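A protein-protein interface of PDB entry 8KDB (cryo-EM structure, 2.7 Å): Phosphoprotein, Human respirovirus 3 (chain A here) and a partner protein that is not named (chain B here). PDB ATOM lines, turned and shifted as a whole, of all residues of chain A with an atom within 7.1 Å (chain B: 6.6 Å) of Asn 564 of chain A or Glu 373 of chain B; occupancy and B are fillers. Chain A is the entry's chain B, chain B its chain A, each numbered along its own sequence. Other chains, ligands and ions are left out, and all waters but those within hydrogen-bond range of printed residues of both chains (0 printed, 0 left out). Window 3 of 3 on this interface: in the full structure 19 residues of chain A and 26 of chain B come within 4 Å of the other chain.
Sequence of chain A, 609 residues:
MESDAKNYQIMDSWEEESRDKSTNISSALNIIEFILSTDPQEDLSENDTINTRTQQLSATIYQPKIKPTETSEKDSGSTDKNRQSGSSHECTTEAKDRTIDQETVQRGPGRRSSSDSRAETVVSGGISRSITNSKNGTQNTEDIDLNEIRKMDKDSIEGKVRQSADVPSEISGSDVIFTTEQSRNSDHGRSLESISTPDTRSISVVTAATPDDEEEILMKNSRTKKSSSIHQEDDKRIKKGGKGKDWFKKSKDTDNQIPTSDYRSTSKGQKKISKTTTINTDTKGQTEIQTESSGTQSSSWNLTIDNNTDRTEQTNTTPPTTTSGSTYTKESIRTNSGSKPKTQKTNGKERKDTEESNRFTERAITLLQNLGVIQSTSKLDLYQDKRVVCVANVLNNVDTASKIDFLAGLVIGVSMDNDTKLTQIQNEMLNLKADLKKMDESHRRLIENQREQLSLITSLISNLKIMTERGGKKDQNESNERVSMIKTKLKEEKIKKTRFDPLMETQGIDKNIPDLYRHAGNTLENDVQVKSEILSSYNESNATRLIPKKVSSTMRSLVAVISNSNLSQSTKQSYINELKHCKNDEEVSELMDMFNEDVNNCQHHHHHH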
ATOM      1  N   LEU A 558      31.018  14.722   6.295  1.00  0.00           N
ATOM      2  CA  LEU A 558      31.637  15.954   5.817  1.00  0.00           C
ATOM      3  C   LEU A 558      32.277  15.755   4.449  1.00  0.00           C
ATOM      4  O   LEU A 558      32.178  16.629   3.578  1.00  0.00           O
ATOM      5  CB  LEU A 558      32.672  16.446   6.827  1.00  0.00           C
ATOM      6  CG  LEU A 558      32.116  16.939   8.163  1.00  0.00           C
ATOM      7  CD1 LEU A 558      33.243  17.270   9.120  1.00  0.00           C
ATOM      8  CD2 LEU A 558      31.203  18.136   7.964  1.00  0.00           C
ATOM      9  N   VAL A 559      32.940  14.615   4.242  1.00  0.00           N
ATOM     10  CA  VAL A 559      33.544  14.334   2.942  1.00  0.00           C
ATOM     11  C   VAL A 559      32.471  14.257   1.865  1.00  0.00           C
ATOM     12  O   VAL A 559      32.637  14.790   0.761  1.00  0.00           O
ATOM     13  CB  VAL A 559      34.381  13.044   3.006  1.00  0.00           C
ATOM     14  CG1 VAL A 559      34.654  12.515   1.608  1.00  0.00           C
ATOM     15  CG2 VAL A 559      35.683  13.293   3.743  1.00  0.00           C
ATOM     16  N   ALA A 560      31.347  13.604   2.171  1.00  0.00           N
ATOM     17  CA  ALA A 560      30.262  13.503   1.199  1.00  0.00           C
ATOM     18  C   ALA A 560      29.633  14.862   0.921  1.00  0.00           C
ATOM     19  O   ALA A 560      29.242  15.147  -0.218  1.00  0.00           O
ATOM     20  CB  ALA A 560      29.209  12.512   1.689  1.00  0.00           C
ATOM     21  N   VAL A 561      29.515  15.709   1.945  1.00  0.00           N
ATOM     22  CA  VAL A 561      28.975  17.051   1.743  1.00  0.00           C
ATOM     23  C   VAL A 561      29.892  17.862   0.838  1.00  0.00           C
ATOM     24  O   VAL A 561      29.431  18.560  -0.074  1.00  0.00           O
ATOM     25  CB  VAL A 561      28.755  17.750   3.099  1.00  0.00           C
ATOM     26  CG1 VAL A 561      28.654  19.255   2.915  1.00  0.00           C
ATOM     27  CG2 VAL A 561      27.508  17.212   3.776  1.00  0.00           C
ATOM     28  N   ILE A 562      31.202  17.778   1.071  1.00  0.00           N
ATOM     29  CA  ILE A 562      32.155  18.507   0.237  1.00  0.00           C
ATOM     30  C   ILE A 562      32.117  17.988  -1.195  1.00  0.00           C
ATOM     31  O   ILE A 562      32.161  18.766  -2.156  1.00  0.00           O
ATOM     32  CB  ILE A 562      33.571  18.415   0.837  1.00  0.00           C
ATOM     33  CG1 ILE A 562      33.671  19.266   2.102  1.00  0.00           C
ATOM     34  CG2 ILE A 562      34.615  18.857  -0.174  1.00  0.00           C
ATOM     35  CD1 ILE A 562      34.893  18.966   2.936  1.00  0.00           C
ATOM     36  N   SER A 563      32.029  16.667  -1.362  1.00  0.00           N
ATOM     37  CA  SER A 563      32.059  16.077  -2.698  1.00  0.00           C
ATOM     38  C   SER A 563      30.863  16.517  -3.533  1.00  0.00           C
ATOM     39  O   SER A 563      31.006  16.815  -4.724  1.00  0.00           O
ATOM     40  CB  SER A 563      32.106  14.554  -2.593  1.00  0.00           C
ATOM     41  OG  SER A 563      33.202  14.131  -1.802  1.00  0.00           O
ATOM     42  N   ASN A 564      29.676  16.562  -2.930  1.00  0.00           N
ATOM     43  CA  ASN A 564      28.446  16.892  -3.636  1.00  0.00           C
ATOM     44  C   ASN A 564      28.221  18.394  -3.768  1.00  0.00           C
ATOM     45  O   ASN A 564      27.099  18.817  -4.065  1.00  0.00           O
ATOM     46  CB  ASN A 564      27.248  16.247  -2.936  1.00  0.00           C
ATOM     47  CG  ASN A 564      27.168  14.754  -3.173  1.00  0.00           C
ATOM     48  OD1 ASN A 564      26.554  14.299  -4.138  1.00  0.00           O
ATOM     49  ND2 ASN A 564      27.786  13.981  -2.290  1.00  0.00           N
ATOM     50  N   SER A 565      29.253  19.206  -3.559  1.00  0.00           N
ATOM     51  CA  SER A 565      29.102  20.651  -3.591  1.00  0.00           C
ATOM     52  C   SER A 565      29.174  21.161  -5.029  1.00  0.00           C
ATOM     53  O   SER A 565      29.260  20.393  -5.989  1.00  0.00           O
ATOM     54  CB  SER A 565      30.159  21.316  -2.712  1.00  0.00           C
ATOM     55  OG  SER A 565      31.423  21.320  -3.347  1.00  0.00           O
ATOM     56  N   ASN A 566      29.134  22.485  -5.178  1.00  0.00           N
ATOM     57  CA  ASN A 566      29.102  23.127  -6.484  1.00  0.00           C
ATOM     58  C   ASN A 566      30.447  23.780  -6.802  1.00  0.00           C
ATOM     59  O   ASN A 566      30.578  24.482  -7.809  1.00  0.00           O
ATOM     60  CB  ASN A 566      27.955  24.150  -6.507  1.00  0.00           C
ATOM     61  CG  ASN A 566      27.667  24.722  -7.893  1.00  0.00           C
ATOM     62  OD1 ASN A 566      28.322  24.394  -8.881  1.00  0.00           O
ATOM     63  ND2 ASN A 566      26.672  25.599  -7.960  1.00  0.00           N
ATOM     64  N   LEU A 567      31.457  23.557  -5.967  1.00  0.00           N
ATOM     65  CA  LEU A 567      32.764  24.156  -6.175  1.00  0.00           C
ATOM     66  C   LEU A 567      33.515  23.438  -7.296  1.00  0.00           C
ATOM     67  O   LEU A 567      33.082  22.409  -7.817  1.00  0.00           O
ATOM     68  CB  LEU A 567      33.581  24.122  -4.885  1.00  0.00           C
ATOM     69  CG  LEU A 567      32.907  24.663  -3.625  1.00  0.00           C
ATOM     70  CD1 LEU A 567      33.861  24.611  -2.445  1.00  0.00           C
ATOM     71  CD2 LEU A 567      32.407  26.078  -3.850  1.00  0.00           C
ATOM     72  N   GLN A 569      36.565  21.252  -9.062  1.00  0.00           N
ATOM     73  CA  GLN A 569      37.103  19.954  -8.669  1.00  0.00           C
ATOM     74  C   GLN A 569      38.387  20.100  -7.862  1.00  0.00           C
ATOM     75  O   GLN A 569      38.600  19.370  -6.886  1.00  0.00           O
ATOM     76  CB  GLN A 569      37.341  19.089  -9.906  1.00  0.00           C
ATOM     77  CG  GLN A 569      36.236  18.084 -10.179  1.00  0.00           C
ATOM     78  CD  GLN A 569      36.235  16.926  -9.199  1.00  0.00           C
ATOM     79  OE1 GLN A 569      37.135  16.795  -8.370  1.00  0.00           O
ATOM     80  NE2 GLN A 569      35.220  16.076  -9.292  1.00  0.00           N
ATOM     81  N   LYS A 572      37.545  21.090  -4.341  1.00  0.00           N
ATOM     82  CA  LYS A 572      36.993  19.945  -3.625  1.00  0.00           C
ATOM     83  C   LYS A 572      38.098  18.995  -3.186  1.00  0.00           C
ATOM     84  O   LYS A 572      38.118  18.534  -2.039  1.00  0.00           O
ATOM     85  CB  LYS A 572      35.987  19.209  -4.508  1.00  0.00           C
ATOM     86  CG  LYS A 572      34.690  19.948  -4.763  1.00  0.00           C
ATOM     87  CD  LYS A 572      33.813  19.157  -5.719  1.00  0.00           C
ATOM     88  CE  LYS A 572      32.497  19.862  -5.981  1.00  0.00           C
ATOM     89  NZ  LYS A 572      31.476  18.938  -6.543  1.00  0.00           N
ATOM     90  N   ILE A 576      39.118  18.057   0.658  1.00  0.00           N
ATOM     91  CA  ILE A 576      39.069  16.672   1.119  1.00  0.00           C
ATOM     92  C   ILE A 576      40.430  16.234   1.647  1.00  0.00           C
ATOM     93  O   ILE A 576      40.521  15.533   2.663  1.00  0.00           O
ATOM     94  CB  ILE A 576      38.566  15.749  -0.006  1.00  0.00           C
ATOM     95  CG1 ILE A 576      37.131  16.114  -0.389  1.00  0.00           C
ATOM     96  CG2 ILE A 576      38.643  14.293   0.412  1.00  0.00           C
ATOM     97  CD1 ILE A 576      36.645  15.440  -1.649  1.00  0.00           C
ATOM     98  N   PHE A 595      35.031  26.314   4.192  1.00  0.00           N
ATOM     99  CA  PHE A 595      34.274  25.688   3.112  1.00  0.00           C
ATOM    100  C   PHE A 595      32.896  26.319   2.966  1.00  0.00           C
ATOM    101  O   PHE A 595      32.424  26.547   1.845  1.00  0.00           O
ATOM    102  CB  PHE A 595      34.147  24.186   3.355  1.00  0.00           C
ATOM    103  CG  PHE A 595      33.130  23.514   2.473  1.00  0.00           C
ATOM    104  CD1 PHE A 595      33.423  23.226   1.153  1.00  0.00           C
ATOM    105  CD2 PHE A 595      31.882  23.176   2.965  1.00  0.00           C
ATOM    106  CE1 PHE A 595      32.489  22.611   0.342  1.00  0.00           C
ATOM    107  CE2 PHE A 595      30.945  22.562   2.160  1.00  0.00           C
ATOM    108  CZ  PHE A 595      31.250  22.278   0.846  1.00  0.00           C
ATOM    109  N   LYS B 290      24.130   2.915 -12.746  1.00  0.00           N
ATOM    110  CA  LYS B 290      24.090   3.041 -11.292  1.00  0.00           C
ATOM    111  C   LYS B 290      23.307   1.898 -10.656  1.00  0.00           C
ATOM    112  O   LYS B 290      23.732   1.336  -9.642  1.00  0.00           O
ATOM    113  CB  LYS B 290      23.502   4.394 -10.896  1.00  0.00           C
ATOM    114  CG  LYS B 290      24.380   5.567 -11.286  1.00  0.00           C
ATOM    115  CD  LYS B 290      23.851   6.874 -10.730  1.00  0.00           C
ATOM    116  CE  LYS B 290      24.778   8.023 -11.077  1.00  0.00           C
ATOM    117  NZ  LYS B 290      26.185   7.728 -10.698  1.00  0.00           N
ATOM    118  N   LEU B 323      21.373  12.087   1.131  1.00  0.00           N
ATOM    119  CA  LEU B 323      22.165  12.562   0.003  1.00  0.00           C
ATOM    120  C   LEU B 323      21.485  13.736  -0.686  1.00  0.00           C
ATOM    121  O   LEU B 323      22.155  14.671  -1.138  1.00  0.00           O
ATOM    122  CB  LEU B 323      22.411  11.423  -0.985  1.00  0.00           C
ATOM    123  CG  LEU B 323      23.515  10.441  -0.594  1.00  0.00           C
ATOM    124  CD1 LEU B 323      23.820   9.492  -1.738  1.00  0.00           C
ATOM    125  CD2 LEU B 323      24.763  11.187  -0.161  1.00  0.00           C
ATOM    126  N   THR B 326      22.026  16.878   1.531  1.00  0.00           N
ATOM    127  CA  THR B 326      23.342  17.521   1.527  1.00  0.00           C
ATOM    128  C   THR B 326      23.437  18.713   0.577  1.00  0.00           C
ATOM    129  O   THR B 326      24.495  19.347   0.520  1.00  0.00           O
ATOM    130  CB  THR B 326      24.453  16.527   1.162  1.00  0.00           C
ATOM    131  OG1 THR B 326      24.353  16.167  -0.221  1.00  0.00           O
ATOM    132  CG2 THR B 326      24.400  15.287   2.032  1.00  0.00           C
ATOM    133  N   HIS B 327      22.380  19.034  -0.166  1.00  0.00           N
ATOM    134  CA  HIS B 327      22.402  20.131  -1.126  1.00  0.00           C
ATOM    135  C   HIS B 327      21.711  21.399  -0.634  1.00  0.00           C
ATOM    136  O   HIS B 327      21.594  22.352  -1.410  1.00  0.00           O
ATOM    137  CB  HIS B 327      21.742  19.699  -2.441  1.00  0.00           C
ATOM    138  CG  HIS B 327      22.556  18.735  -3.246  1.00  0.00           C
ATOM    139  ND1 HIS B 327      22.580  17.382  -2.988  1.00  0.00           N
ATOM    140  CD2 HIS B 327      23.362  18.928  -4.317  1.00  0.00           C
ATOM    141  CE1 HIS B 327      23.372  16.783  -3.859  1.00  0.00           C
ATOM    142  NE2 HIS B 327      23.859  17.699  -4.676  1.00  0.00           N
ATOM    143  N   ASP B 369      30.183   5.857  -3.105  1.00  0.00           N
ATOM    144  CA  ASP B 369      30.788   6.457  -4.289  1.00  0.00           C
ATOM    145  C   ASP B 369      30.014   6.171  -5.571  1.00  0.00           C
ATOM    146  O   ASP B 369      30.324   6.774  -6.603  1.00  0.00           O
ATOM    147  CB  ASP B 369      32.244   6.000  -4.432  1.00  0.00           C
ATOM    148  CG  ASP B 369      32.380   4.509  -4.689  1.00  0.00           C
ATOM    149  OD1 ASP B 369      31.355   3.811  -4.819  1.00  0.00           O
ATOM    150  OD2 ASP B 369      33.532   4.031  -4.763  1.00  0.00           O
ATOM    151  N   ILE B 370      29.036   5.267  -5.535  1.00  0.00           N
ATOM    152  CA  ILE B 370      28.191   5.050  -6.705  1.00  0.00           C
ATOM    153  C   ILE B 370      27.369   6.294  -7.010  1.00  0.00           C
ATOM    154  O   ILE B 370      27.245   6.703  -8.170  1.00  0.00           O
ATOM    155  CB  ILE B 370      27.290   3.820  -6.490  1.00  0.00           C
ATOM    156  CG1 ILE B 370      28.127   2.548  -6.371  1.00  0.00           C
ATOM    157  CG2 ILE B 370      26.288   3.686  -7.625  1.00  0.00           C
ATOM    158  CD1 ILE B 370      27.317   1.329  -6.005  1.00  0.00           C
ATOM    159  N   PHE B 371      26.800   6.919  -5.980  1.00  0.00           N
ATOM    160  CA  PHE B 371      25.806   7.969  -6.158  1.00  0.00           C
ATOM    161  C   PHE B 371      26.343   9.367  -5.879  1.00  0.00           C
ATOM    162  O   PHE B 371      25.561  10.323  -5.856  1.00  0.00           O
ATOM    163  CB  PHE B 371      24.593   7.686  -5.273  1.00  0.00           C
ATOM    164  CG  PHE B 371      23.766   6.534  -5.751  1.00  0.00           C
ATOM    165  CD1 PHE B 371      23.011   6.637  -6.905  1.00  0.00           C
ATOM    166  CD2 PHE B 371      23.760   5.336  -5.057  1.00  0.00           C
ATOM    167  CE1 PHE B 371      22.259   5.573  -7.354  1.00  0.00           C
ATOM    168  CE2 PHE B 371      23.008   4.270  -5.499  1.00  0.00           C
ATOM    169  CZ  PHE B 371      22.259   4.387  -6.649  1.00  0.00           C
ATOM    170  N   ASN B 372      27.647   9.514  -5.669  1.00  0.00           N
ATOM    171  CA  ASN B 372      28.225  10.822  -5.404  1.00  0.00           C
ATOM    172  C   ASN B 372      28.322  11.640  -6.687  1.00  0.00           C
ATOM    173  O   ASN B 372      28.515  11.099  -7.779  1.00  0.00           O
ATOM    174  CB  ASN B 372      29.607  10.680  -4.768  1.00  0.00           C
ATOM    175  CG  ASN B 372      29.543  10.561  -3.257  1.00  0.00           C
ATOM    176  OD1 ASN B 372      28.476  10.336  -2.686  1.00  0.00           O
ATOM    177  ND2 ASN B 372      30.687  10.713  -2.602  1.00  0.00           N
ATOM    178  N   GLU B 373      28.186  12.961  -6.538  1.00  0.00           N
ATOM    179  CA  GLU B 373      28.209  13.895  -7.668  1.00  0.00           C
ATOM    180  C   GLU B 373      27.162  13.532  -8.718  1.00  0.00           C
ATOM    181  O   GLU B 373      27.430  13.535  -9.921  1.00  0.00           O
ATOM    182  CB  GLU B 373      29.603  13.975  -8.295  1.00  0.00           C
ATOM    183  CG  GLU B 373      30.660  14.582  -7.389  1.00  0.00           C
ATOM    184  CD  GLU B 373      32.023  14.653  -8.050  1.00  0.00           C
ATOM    185  OE1 GLU B 373      32.161  14.150  -9.186  1.00  0.00           O
ATOM    186  OE2 GLU B 373      32.956  15.209  -7.435  1.00  0.00           O
ATOM    187  N   SER B 374      25.957  13.211  -8.258  1.00  0.00           N
ATOM    188  CA  SER B 374      24.850  12.860  -9.131  1.00  0.00           C
ATOM    189  C   SER B 374      23.685  13.813  -8.900  1.00  0.00           C
ATOM    190  O   SER B 374      23.565  14.437  -7.844  1.00  0.00           O
ATOM    191  CB  SER B 374      24.406  11.409  -8.907  1.00  0.00           C
ATOM    192  OG  SER B 374      23.753  11.263  -7.661  1.00  0.00           O
ATOM    193  N   THR B 375      22.827  13.921  -9.911  1.00  0.00           N
ATOM    194  CA  THR B 375      21.729  14.874  -9.878  1.00  0.00           C
ATOM    195  C   THR B 375      20.679  14.459  -8.849  1.00  0.00           C
ATOM    196  O   THR B 375      20.674  13.337  -8.335  1.00  0.00           O
ATOM    197  CB  THR B 375      21.090  15.007 -11.259  1.00  0.00           C
ATOM    198  OG1 THR B 375      20.586  13.733 -11.680  1.00  0.00           O
ATOM    199  CG2 THR B 375      22.111  15.499 -12.269  1.00  0.00           C
ATOM    200  N   GLU B 378      18.448  11.581 -10.084  1.00  0.00           N
ATOM    201  CA  GLU B 378      19.117  10.287 -10.013  1.00  0.00           C
ATOM    202  C   GLU B 378      19.075   9.722  -8.599  1.00  0.00           C
ATOM    203  O   GLU B 378      18.796   8.533  -8.406  1.00  0.00           O
ATOM    204  CB  GLU B 378      20.558  10.422 -10.498  1.00  0.00           C
ATOM    205  CG  GLU B 378      20.695  10.447 -12.007  1.00  0.00           C
ATOM    206  CD  GLU B 378      22.048  10.954 -12.460  1.00  0.00           C
ATOM    207  OE1 GLU B 378      23.053  10.656 -11.783  1.00  0.00           O
ATOM    208  OE2 GLU B 378      22.107  11.656 -13.490  1.00  0.00           O
ATOM    209  N   ILE B 379      19.346  10.559  -7.596  1.00  0.00           N
ATOM    210  CA  ILE B 379      19.283  10.100  -6.212  1.00  0.00           C
ATOM    211  C   ILE B 379      17.854   9.735  -5.837  1.00  0.00           C
ATOM    212  O   ILE B 379      17.619   8.781  -5.089  1.00  0.00           O
ATOM    213  CB  ILE B 379      19.862  11.168  -5.266  1.00  0.00           C
ATOM    214  CG1 ILE B 379      21.309  11.484  -5.632  1.00  0.00           C
ATOM    215  CG2 ILE B 379      19.791  10.702  -3.826  1.00  0.00           C
ATOM    216  CD1 ILE B 379      21.842  12.725  -4.961  1.00  0.00           C
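The backbone NH (N) of Glu 373 of chain B lies within hydrogen-bond range of the side-chain amide oxygen (OD1) of Asn 564 of chain A, at 3.2 Å. The side-chain amide nitrogen (NE2) of Gln 569 of chain A is in hydrogen-bond range of the side-chain carboxylate (OE2) of Glu 373 of chain B. O of Asn 564 of chain A sits at hydrogen-bond distance from NE2 of His 327 of chain B (3.5 Å).
O of Ala 560 of chain A is in hydrogen-bond range of ND2 of Asn 564 of chain A, 2.8 Å away. A ring nitrogen (ND1) of His 327 of chain B lies within hydrogen-bond range of the backbone carbonyl oxygen (O) of Leu 323 of chain B (3.3 Å). O of Ser 563 of chain A lies within hydrogen-bond range of NZ of Lys 572 of chain A. The backbone carbonyl oxygen (O) of Val 559 of chain A sits at hydrogen-bond distance from the side-chain hydroxyl (OG) of Ser 563 of chain A (2.7 Å). The side-chain hydroxyl (OG1) of Thr 326 of chain B is in hydrogen-bond range of the backbone carbonyl oxygen (O) of Leu 323 of chain B, 2.8 Å away.
Among the printed residues, merely in contact across the chains: Ser 563 of chain A with Glu 373 of chain B (3.5 Å), Asn 564 of chain A with Asn 372 of chain B (3.7 Å) and Asn 564 of chain A with Thr 326 of chain B (3.97 Å).
Of the printed residues of chain B, Ser 563 of chain A touches Glu 373 (3.5 Å). Printed residues of chain B within 4 Å of Asn 564 of chain A: Thr 326 (3.97 Å), His 327 (3.5 Å), Asn 372 (3.7 Å) and Glu 373 (3.2 Å). Of the printed residues of chain B, Gln 569 of chain A touches Glu 373 (3.1 Å). Printed residues of chain A within 4 Å of Thr 326 of chain B: Asn 564 (3.97 Å). Printed residues of chain A within 4 Å of His 327 of chain B: Asn 564 (3.5 Å). Printed residues of chain A within 4 Å of Asn 372 of chain B: Asn 564 (3.7 Å). Glu 373 of chain B touches just these residues of chain A: Ser 563 (3.5 Å), Asn 564 (3.2 Å) and Gln 569 (3.1 Å). The nearest printed residue of chain B that does not touch Asn 564 of chain A is Ser 374 of chain B (4.3 Å). The nearest residue of chain A that does not touch Glu 373 of chain B is Lys 572 of chain A (4.1 Å). The nearest printed residue of chain B that does not touch Gln 569 of chain A is Asn 372 of chain B (8.5 Å).
Of the 13 printed residues of chain B, 4 touch a printed residue of chain A. Hydrophobic or aromatic side chains of chain B within 4 Å of the printed part of chain A: His 327. Among the printed residues, 6 pairs touch across the chains. Among the printed residues, no Asp or Glu carboxylate lies within 4 Å of a Lys or Arg side-chain nitrogen of the other chain.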
